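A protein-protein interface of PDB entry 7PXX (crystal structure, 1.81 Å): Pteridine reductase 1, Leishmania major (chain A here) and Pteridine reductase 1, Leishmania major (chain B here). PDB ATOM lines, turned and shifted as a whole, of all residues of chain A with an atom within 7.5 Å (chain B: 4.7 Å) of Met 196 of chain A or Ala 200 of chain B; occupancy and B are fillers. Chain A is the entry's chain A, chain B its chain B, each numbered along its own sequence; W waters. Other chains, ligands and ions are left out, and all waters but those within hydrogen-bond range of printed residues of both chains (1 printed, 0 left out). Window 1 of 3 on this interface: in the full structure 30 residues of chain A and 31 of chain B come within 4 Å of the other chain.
Of the 19 printed residues of chain A, 7 touch a printed residue of chain B. Among the printed residues, 12 pairs touch across the chains. Among the printed residues, no Asp or Glu carboxylate lies within 4 Å of a Lys or Arg side-chain nitrogen of the other chain.
Thr 116 of chain A touches Tyr 152 of chain B. O of Ala 148 of chain A touches CE of Met 196 of chain B (3.3 Å). Thr 192 of chain A touches Tyr 152 of chain B (CG2 to CD1, 3.6 Å). Thr 192 of chain A touches Leu 204 of chain B. CE2 of Tyr 152 of chain B touches CD1 of Ile 193 of chain A, 3.4 Å away. CE of Met 196 of chain A touches O of Ala 148 of chain B, 3.5 Å away. Ala 200 of chain B touches Met 196 of chain A. N of Leu 204 of chain B touches CG of Met 196 of chain A (3.8 Å). Gly 199 of chain A touches Gly 199 of chain B. Ala 200 of chain A touches Ala 200 of chain B.
OG1 of Thr 116 of chain A lies within hydrogen-bond range of N of Thr 192 of chain A. The backbone NH of Ile 193 of chain A is in hydrogen-bond range of the side-chain hydroxyl of Thr 116 of chain A (3.1 Å).
Of the printed residues of chain B, Met 196 of chain A touches Ala 148 (3.5 Å), Ala 200 (3.3 Å) and Leu 204 (3.8 Å). Of the printed residues of chain A, Met 196 of chain B touches Ala 148 (3.3 Å) and Ala 200 (3.3 Å). Printed residues of chain B within 4 Å of Ile 193 of chain A: Tyr 152. Of the printed residues of chain B, Gly 199 of chain A touches Gly 199 (3.7 Å). Of the printed residues of chain A, Leu 204 of chain B touches Thr 192 and Met 196. Printed residues of chain B within 4 Å of Thr 116 of chain A: Tyr 152 (3.6 Å). The nearest residue of chain B that does not touch Met 196 of chain A is Tyr 152 of chain B (4.02 Å). The nearest printed residue of chain A that does not touch Ala 200 of chain B is Gly 199 of chain A (4.02 Å). The nearest printed residue of chain A that does not touch Met 196 of chain B is Gly 203 of chain A (4.3 Å).
Water W1 lies within hydrogen-bond range of the side-chain hydroxyl (OH) of Tyr 152 of chain B (2.9 Å) and the backbone carbonyl oxygen (O) of Thr 116 of chain A (3.1 Å).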
ATOM      1  N   THR A 116      30.900   4.223  31.964  1.00  0.00           N
ATOM      2  CA  THR A 116      29.618   3.519  31.904  1.00  0.00           C
ATOM      3  C   THR A 116      29.733   2.407  30.871  1.00  0.00           C
ATOM      4  O   THR A 116      29.216   2.533  29.755  1.00  0.00           O
ATOM      5  CB  THR A 116      28.476   4.454  31.519  1.00  0.00           C
ATOM      6  OG1 THR A 116      28.839   5.145  30.320  1.00  0.00           O
ATOM      7  CG2 THR A 116      28.248   5.463  32.617  1.00  0.00           C
ATOM      8  N   LEU A 143      26.220  12.414  34.622  1.00  0.00           N
ATOM      9  CA  LEU A 143      27.068  12.654  33.459  1.00  0.00           C
ATOM     10  C   LEU A 143      26.336  13.498  32.422  1.00  0.00           C
ATOM     11  O   LEU A 143      26.904  14.447  31.869  1.00  0.00           O
ATOM     12  CB  LEU A 143      27.517  11.322  32.865  1.00  0.00           C
ATOM     13  CG  LEU A 143      28.465  10.460  33.689  1.00  0.00           C
ATOM     14  CD1 LEU A 143      28.482   9.037  33.123  1.00  0.00           C
ATOM     15  CD2 LEU A 143      29.872  11.044  33.678  1.00  0.00           C
ATOM     16  N   PHE A 144      25.065  13.194  32.158  1.00  0.00           N
ATOM     17  CA  PHE A 144      24.358  13.974  31.145  1.00  0.00           C
ATOM     18  C   PHE A 144      24.026  15.368  31.656  1.00  0.00           C
ATOM     19  O   PHE A 144      24.012  16.331  30.881  1.00  0.00           O
ATOM     20  CB  PHE A 144      23.085  13.252  30.704  1.00  0.00           C
ATOM     21  CG  PHE A 144      23.244  12.450  29.451  1.00  0.00           C
ATOM     22  CD1 PHE A 144      23.890  12.981  28.346  1.00  0.00           C
ATOM     23  CD2 PHE A 144      22.744  11.151  29.372  1.00  0.00           C
ATOM     24  CE1 PHE A 144      24.041  12.246  27.191  1.00  0.00           C
ATOM     25  CE2 PHE A 144      22.881  10.396  28.200  1.00  0.00           C
ATOM     26  CZ  PHE A 144      23.540  10.939  27.113  1.00  0.00           C
ATOM     27  N   ASN A 147      27.380  17.709  31.809  1.00  0.00           N
ATOM     28  CA  ASN A 147      28.087  17.930  30.557  1.00  0.00           C
ATOM     29  C   ASN A 147      27.194  18.466  29.443  1.00  0.00           C
ATOM     30  O   ASN A 147      27.723  18.957  28.432  1.00  0.00           O
ATOM     31  CB  ASN A 147      28.731  16.624  30.082  1.00  0.00           C
ATOM     32  CG  ASN A 147      29.954  16.229  30.895  1.00  0.00           C
ATOM     33  OD1 ASN A 147      31.036  16.790  30.722  1.00  0.00           O
ATOM     34  ND2 ASN A 147      29.797  15.217  31.743  1.00  0.00           N
ATOM     35  N   ALA A 148      25.866  18.400  29.590  1.00  0.00           N
ATOM     36  CA  ALA A 148      25.020  18.800  28.472  1.00  0.00           C
ATOM     37  C   ALA A 148      23.771  19.573  28.873  1.00  0.00           C
ATOM     38  O   ALA A 148      23.543  20.685  28.375  1.00  0.00           O
ATOM     39  CB  ALA A 148      24.621  17.569  27.659  1.00  0.00           C
ATOM     40  N   THR A 184      36.658  13.509  20.434  1.00  0.00           N
ATOM     41  CA  THR A 184      35.266  13.088  20.294  1.00  0.00           C
ATOM     42  C   THR A 184      35.100  12.011  19.225  1.00  0.00           C
ATOM     43  O   THR A 184      34.307  11.079  19.406  1.00  0.00           O
ATOM     44  CB  THR A 184      34.375  14.302  19.995  1.00  0.00           C
ATOM     45  OG1 THR A 184      32.995  13.913  20.016  1.00  0.00           O
ATOM     46  CG2 THR A 184      34.728  14.950  18.644  1.00  0.00           C
ATOM     47  N   TYR A 191      33.369   4.669  28.133  1.00  0.00           N
ATOM     48  CA  TYR A 191      32.881   5.964  28.599  1.00  0.00           C
ATOM     49  C   TYR A 191      31.698   6.488  27.777  1.00  0.00           C
ATOM     50  O   TYR A 191      31.630   7.684  27.494  1.00  0.00           O
ATOM     51  CB  TYR A 191      34.009   6.990  28.584  1.00  0.00           C
ATOM     52  CG  TYR A 191      34.976   6.871  29.755  1.00  0.00           C
ATOM     53  CD1 TYR A 191      35.840   5.794  29.855  1.00  0.00           C
ATOM     54  CD2 TYR A 191      35.018   7.844  30.746  1.00  0.00           C
ATOM     55  CE1 TYR A 191      36.730   5.687  30.918  1.00  0.00           C
ATOM     56  CE2 TYR A 191      35.896   7.745  31.820  1.00  0.00           C
ATOM     57  CZ  TYR A 191      36.746   6.663  31.905  1.00  0.00           C
ATOM     58  OH  TYR A 191      37.631   6.553  32.972  1.00  0.00           O
ATOM     59  N   THR A 192      30.715   5.618  27.462  1.00  0.00           N
ATOM     60  CA  THR A 192      29.698   5.945  26.455  1.00  0.00           C
ATOM     61  C   THR A 192      28.837   7.146  26.848  1.00  0.00           C
ATOM     62  O   THR A 192      28.527   7.997  26.000  1.00  0.00           O
ATOM     63  CB  THR A 192      28.820   4.717  26.157  1.00  0.00           C
ATOM     64  OG1 THR A 192      29.595   3.752  25.441  1.00  0.00           O
ATOM     65  CG2 THR A 192      27.607   5.077  25.272  1.00  0.00           C
ATOM     66  N   ILE A 193      28.411   7.243  28.112  1.00  0.00           N
ATOM     67  CA  ILE A 193      27.560   8.380  28.451  1.00  0.00           C
ATOM     68  C   ILE A 193      28.342   9.680  28.382  1.00  0.00           C
ATOM     69  O   ILE A 193      27.839  10.689  27.895  1.00  0.00           O
ATOM     70  CB  ILE A 193      26.899   8.204  29.827  1.00  0.00           C
ATOM     71  CG1 ILE A 193      26.062   6.929  29.846  1.00  0.00           C
ATOM     72  CG2 ILE A 193      25.969   9.383  30.097  1.00  0.00           C
ATOM     73  CD1 ILE A 193      24.820   7.028  29.025  1.00  0.00           C
ATOM     74  N   TYR A 194      29.577   9.686  28.897  1.00  0.00           N
ATOM     75  CA  TYR A 194      30.418  10.865  28.807  1.00  0.00           C
ATOM     76  C   TYR A 194      30.582  11.290  27.353  1.00  0.00           C
ATOM     77  O   TYR A 194      30.315  12.447  26.983  1.00  0.00           O
ATOM     78  CB  TYR A 194      31.790  10.572  29.434  1.00  0.00           C
ATOM     79  CG  TYR A 194      32.790  11.683  29.187  1.00  0.00           C
ATOM     80  CD1 TYR A 194      32.799  12.804  29.996  1.00  0.00           C
ATOM     81  CD2 TYR A 194      33.706  11.618  28.132  1.00  0.00           C
ATOM     82  CE1 TYR A 194      33.689  13.843  29.781  1.00  0.00           C
ATOM     83  CE2 TYR A 194      34.614  12.644  27.919  1.00  0.00           C
ATOM     84  CZ  TYR A 194      34.588  13.764  28.750  1.00  0.00           C
ATOM     85  OH  TYR A 194      35.467  14.806  28.563  1.00  0.00           O
ATOM     86  N   THR A 195      30.960  10.340  26.500  1.00  0.00           N
ATOM     87  CA  THR A 195      31.159  10.665  25.088  1.00  0.00           C
ATOM     88  C   THR A 195      29.884  11.235  24.483  1.00  0.00           C
ATOM     89  O   THR A 195      29.925  12.238  23.769  1.00  0.00           O
ATOM     90  CB  THR A 195      31.596   9.413  24.340  1.00  0.00           C
ATOM     91  OG1 THR A 195      32.705   8.826  25.026  1.00  0.00           O
ATOM     92  CG2 THR A 195      31.976   9.736  22.888  1.00  0.00           C
ATOM     93  N   MET A 196      28.736  10.622  24.796  1.00  0.00           N
ATOM     94  CA  MET A 196      27.446  11.117  24.311  1.00  0.00           C
ATOM     95  C   MET A 196      27.192  12.559  24.760  1.00  0.00           C
ATOM     96  O   MET A 196      26.735  13.404  23.981  1.00  0.00           O
ATOM     97  CB  MET A 196      26.327  10.201  24.828  1.00  0.00           C
ATOM     98  CG  MET A 196      26.324   8.787  24.238  1.00  0.00           C
ATOM     99  SD  MET A 196      24.977   7.817  24.925  1.00  0.00           S
ATOM    100  CE  MET A 196      23.588   8.657  24.109  1.00  0.00           C
ATOM    101  N   ALA A 197      27.416  12.834  26.043  1.00  0.00           N
ATOM    102  CA  ALA A 197      27.146  14.169  26.572  1.00  0.00           C
ATOM    103  C   ALA A 197      28.020  15.228  25.895  1.00  0.00           C
ATOM    104  O   ALA A 197      27.537  16.306  25.537  1.00  0.00           O
ATOM    105  CB  ALA A 197      27.342  14.158  28.085  1.00  0.00           C
ATOM    106  N   LYS A 198      29.307  14.941  25.713  1.00  0.00           N
ATOM    107  CA  LYS A 198      30.164  15.883  25.002  1.00  0.00           C
ATOM    108  C   LYS A 198      29.709  16.057  23.558  1.00  0.00           C
ATOM    109  O   LYS A 198      29.824  17.152  23.000  1.00  0.00           O
ATOM    110  CB  LYS A 198      31.626  15.419  25.045  1.00  0.00           C
ATOM    111  CG  LYS A 198      32.300  15.553  26.415  1.00  0.00           C
ATOM    112  CD  LYS A 198      31.918  16.856  27.121  1.00  0.00           C
ATOM    113  CE  LYS A 198      32.953  17.174  28.167  1.00  0.00           C
ATOM    114  NZ  LYS A 198      32.690  18.450  28.863  1.00  0.00           N
ATOM    115  N   GLY A 199      29.200  14.996  22.935  1.00  0.00           N
ATOM    116  CA  GLY A 199      28.654  15.144  21.594  1.00  0.00           C
ATOM    117  C   GLY A 199      27.427  16.032  21.592  1.00  0.00           C
ATOM    118  O   GLY A 199      27.230  16.851  20.685  1.00  0.00           O
ATOM    119  N   ALA A 200      26.599  15.897  22.623  1.00  0.00           N
ATOM    120  CA  ALA A 200      25.484  16.816  22.816  1.00  0.00           C
ATOM    121  C   ALA A 200      25.964  18.246  23.060  1.00  0.00           C
ATOM    122  O   ALA A 200      25.339  19.199  22.595  1.00  0.00           O
ATOM    123  CB  ALA A 200      24.632  16.326  23.994  1.00  0.00           C
ATOM    124  N   LEU A 201      27.069  18.415  23.800  1.00  0.00           N
ATOM    125  CA  LEU A 201      27.589  19.753  24.089  1.00  0.00           C
ATOM    126  C   LEU A 201      28.109  20.441  22.830  1.00  0.00           C
ATOM    127  O   LEU A 201      27.996  21.668  22.691  1.00  0.00           O
ATOM    128  CB  LEU A 201      28.698  19.660  25.155  1.00  0.00           C
ATOM    129  CG  LEU A 201      29.155  20.980  25.766  1.00  0.00           C
ATOM    130  CD1 LEU A 201      27.938  21.806  26.208  1.00  0.00           C
ATOM    131  CD2 LEU A 201      30.118  20.797  26.923  1.00  0.00           C
ATOM    132  N   GLU A 202      28.673  19.676  21.900  1.00  0.00           N
ATOM    133  CA  GLU A 202      29.040  20.258  20.617  1.00  0.00           C
ATOM    134  C   GLU A 202      27.804  20.687  19.835  1.00  0.00           C
ATOM    135  O   GLU A 202      27.808  21.746  19.214  1.00  0.00           O
ATOM    136  CB  GLU A 202      29.881  19.273  19.811  1.00  0.00           C
ATOM    137  CG  GLU A 202      31.217  19.007  20.457  1.00  0.00           C
ATOM    138  CD  GLU A 202      32.309  18.768  19.452  1.00  0.00           C
ATOM    139  OE1 GLU A 202      32.127  19.153  18.274  1.00  0.00           O
ATOM    140  OE2 GLU A 202      33.347  18.189  19.846  1.00  0.00           O
ATOM    141  N   GLY A 203      26.721  19.903  19.889  1.00  0.00           N
ATOM    142  CA  GLY A 203      25.485  20.343  19.255  1.00  0.00           C
ATOM    143  C   GLY A 203      24.983  21.646  19.844  1.00  0.00           C
ATOM    144  O   GLY A 203      24.561  22.557  19.129  1.00  0.00           O
ATOM    145  N   ALA B 148      18.269   9.721  22.262  1.00  0.00           N
ATOM    146  CA  ALA B 148      19.605   9.472  22.789  1.00  0.00           C
ATOM    147  C   ALA B 148      19.643   8.453  23.926  1.00  0.00           C
ATOM    148  O   ALA B 148      20.358   7.450  23.832  1.00  0.00           O
ATOM    149  CB  ALA B 148      20.233  10.792  23.256  1.00  0.00           C
ATOM    150  N   TYR B 152      20.842   4.533  24.037  1.00  0.00           N
ATOM    151  CA  TYR B 152      21.847   3.998  24.952  1.00  0.00           C
ATOM    152  C   TYR B 152      21.338   2.724  25.630  1.00  0.00           C
ATOM    153  O   TYR B 152      21.955   1.665  25.524  1.00  0.00           O
ATOM    154  CB  TYR B 152      22.236   5.067  25.977  1.00  0.00           C
ATOM    155  CG  TYR B 152      23.132   4.528  27.055  1.00  0.00           C
ATOM    156  CD1 TYR B 152      24.418   4.112  26.762  1.00  0.00           C
ATOM    157  CD2 TYR B 152      22.673   4.393  28.354  1.00  0.00           C
ATOM    158  CE1 TYR B 152      25.241   3.596  27.758  1.00  0.00           C
ATOM    159  CE2 TYR B 152      23.471   3.890  29.338  1.00  0.00           C
ATOM    160  CZ  TYR B 152      24.748   3.489  29.041  1.00  0.00           C
ATOM    161  OH  TYR B 152      25.529   2.988  30.062  1.00  0.00           O
ATOM    162  N   MET B 196      21.138  18.679  20.099  1.00  0.00           N
ATOM    163  CA  MET B 196      21.988  18.083  21.116  1.00  0.00           C
ATOM    164  C   MET B 196      21.797  16.579  21.162  1.00  0.00           C
ATOM    165  O   MET B 196      22.767  15.821  21.266  1.00  0.00           O
ATOM    166  CB  MET B 196      21.670  18.680  22.472  1.00  0.00           C
ATOM    167  CG  MET B 196      22.121  20.103  22.610  1.00  0.00           C
ATOM    168  SD  MET B 196      21.645  20.765  24.185  1.00  0.00           S
ATOM    169  CE  MET B 196      22.761  19.893  25.280  1.00  0.00           C
ATOM    170  N   ALA B 197      20.541  16.134  21.110  1.00  0.00           N
ATOM    171  CA  ALA B 197      20.257  14.713  21.198  1.00  0.00           C
ATOM    172  C   ALA B 197      20.824  13.953  20.002  1.00  0.00           C
ATOM    173  O   ALA B 197      21.365  12.856  20.164  1.00  0.00           O
ATOM    174  CB  ALA B 197      18.746  14.507  21.325  1.00  0.00           C
ATOM    175  N   LYS B 198      20.709  14.508  18.791  1.00  0.00           N
ATOM    176  CA  LYS B 198      21.307  13.847  17.634  1.00  0.00           C
ATOM    177  C   LYS B 198      22.837  13.855  17.716  1.00  0.00           C
ATOM    178  O   LYS B 198      23.497  12.909  17.266  1.00  0.00           O
ATOM    179  CB  LYS B 198      20.818  14.516  16.342  1.00  0.00           C
ATOM    180  CG  LYS B 198      19.359  14.226  15.985  1.00  0.00           C
ATOM    181  CD  LYS B 198      19.074  12.725  15.914  1.00  0.00           C
ATOM    182  CE  LYS B 198      17.692  12.468  15.340  1.00  0.00           C
ATOM    183  NZ  LYS B 198      17.222  11.054  15.446  1.00  0.00           N
ATOM    184  N   GLY B 199      23.419  14.883  18.330  1.00  0.00           N
ATOM    185  CA  GLY B 199      24.852  14.855  18.574  1.00  0.00           C
ATOM    186  C   GLY B 199      25.246  13.765  19.554  1.00  0.00           C
ATOM    187  O   GLY B 199      26.283  13.107  19.385  1.00  0.00           O
ATOM    188  N   ALA B 200      24.427  13.555  20.597  1.00  0.00           N
ATOM    189  CA  ALA B 200      24.712  12.470  21.525  1.00  0.00           C
ATOM    190  C   ALA B 200      24.570  11.127  20.830  1.00  0.00           C
ATOM    191  O   ALA B 200      25.341  10.198  21.100  1.00  0.00           O
ATOM    192  CB  ALA B 200      23.781  12.532  22.741  1.00  0.00           C
ATOM    193  N   LEU B 201      23.593  11.022  19.930  1.00  0.00           N
ATOM    194  CA  LEU B 201      23.379   9.791  19.171  1.00  0.00           C
ATOM    195  C   LEU B 201      24.568   9.469  18.266  1.00  0.00           C
ATOM    196  O   LEU B 201      24.933   8.302  18.090  1.00  0.00           O
ATOM    197  CB  LEU B 201      22.097   9.930  18.343  1.00  0.00           C
ATOM    198  CG  LEU B 201      21.552   8.644  17.739  1.00  0.00           C
ATOM    199  CD1 LEU B 201      21.405   7.570  18.806  1.00  0.00           C
ATOM    200  CD2 LEU B 201      20.233   8.888  17.048  1.00  0.00           C
ATOM    201  N   GLU B 202      25.159  10.480  17.647  1.00  0.00           N
ATOM    202  CA  GLU B 202      26.389  10.222  16.896  1.00  0.00           C
ATOM    203  C   GLU B 202      27.513   9.758  17.813  1.00  0.00           C
ATOM    204  O   GLU B 202      28.336   8.907  17.429  1.00  0.00           O
ATOM    205  CB  GLU B 202      26.808  11.468  16.136  1.00  0.00           C
ATOM    206  CG  GLU B 202      25.876  11.769  15.002  1.00  0.00           C
ATOM    207  CD  GLU B 202      26.515  12.641  13.957  1.00  0.00           C
ATOM    208  OE1 GLU B 202      27.642  13.123  14.198  1.00  0.00           O
ATOM    209  OE2 GLU B 202      25.883  12.855  12.906  1.00  0.00           O
ATOM    210  N   GLY B 203      27.566  10.304  19.034  1.00  0.00           N
ATOM    211  CA  GLY B 203      28.584   9.864  19.970  1.00  0.00           C
ATOM    212  C   GLY B 203      28.351   8.434  20.405  1.00  0.00           C
ATOM    213  O   GLY B 203      29.306   7.665  20.609  1.00  0.00           O
ATOM    214  N   LEU B 204      27.077   8.067  20.572  1.00  0.00           N
ATOM    215  CA  LEU B 204      26.731   6.696  20.922  1.00  0.00           C
ATOM    216  C   LEU B 204      27.145   5.739  19.813  1.00  0.00           C
ATOM    217  O   LEU B 204      27.667   4.649  20.073  1.00  0.00           O
ATOM    218  CB  LEU B 204      25.220   6.598  21.194  1.00  0.00           C
ATOM    219  CG  LEU B 204      24.648   5.204  21.471  1.00  0.00           C
ATOM    220  CD1 LEU B 204      25.392   4.513  22.598  1.00  0.00           C
ATOM    221  CD2 LEU B 204      23.187   5.311  21.834  1.00  0.00           C
HETATM  222  O   HOH W   1      27.157   1.242  31.702  1.00  0.00           O
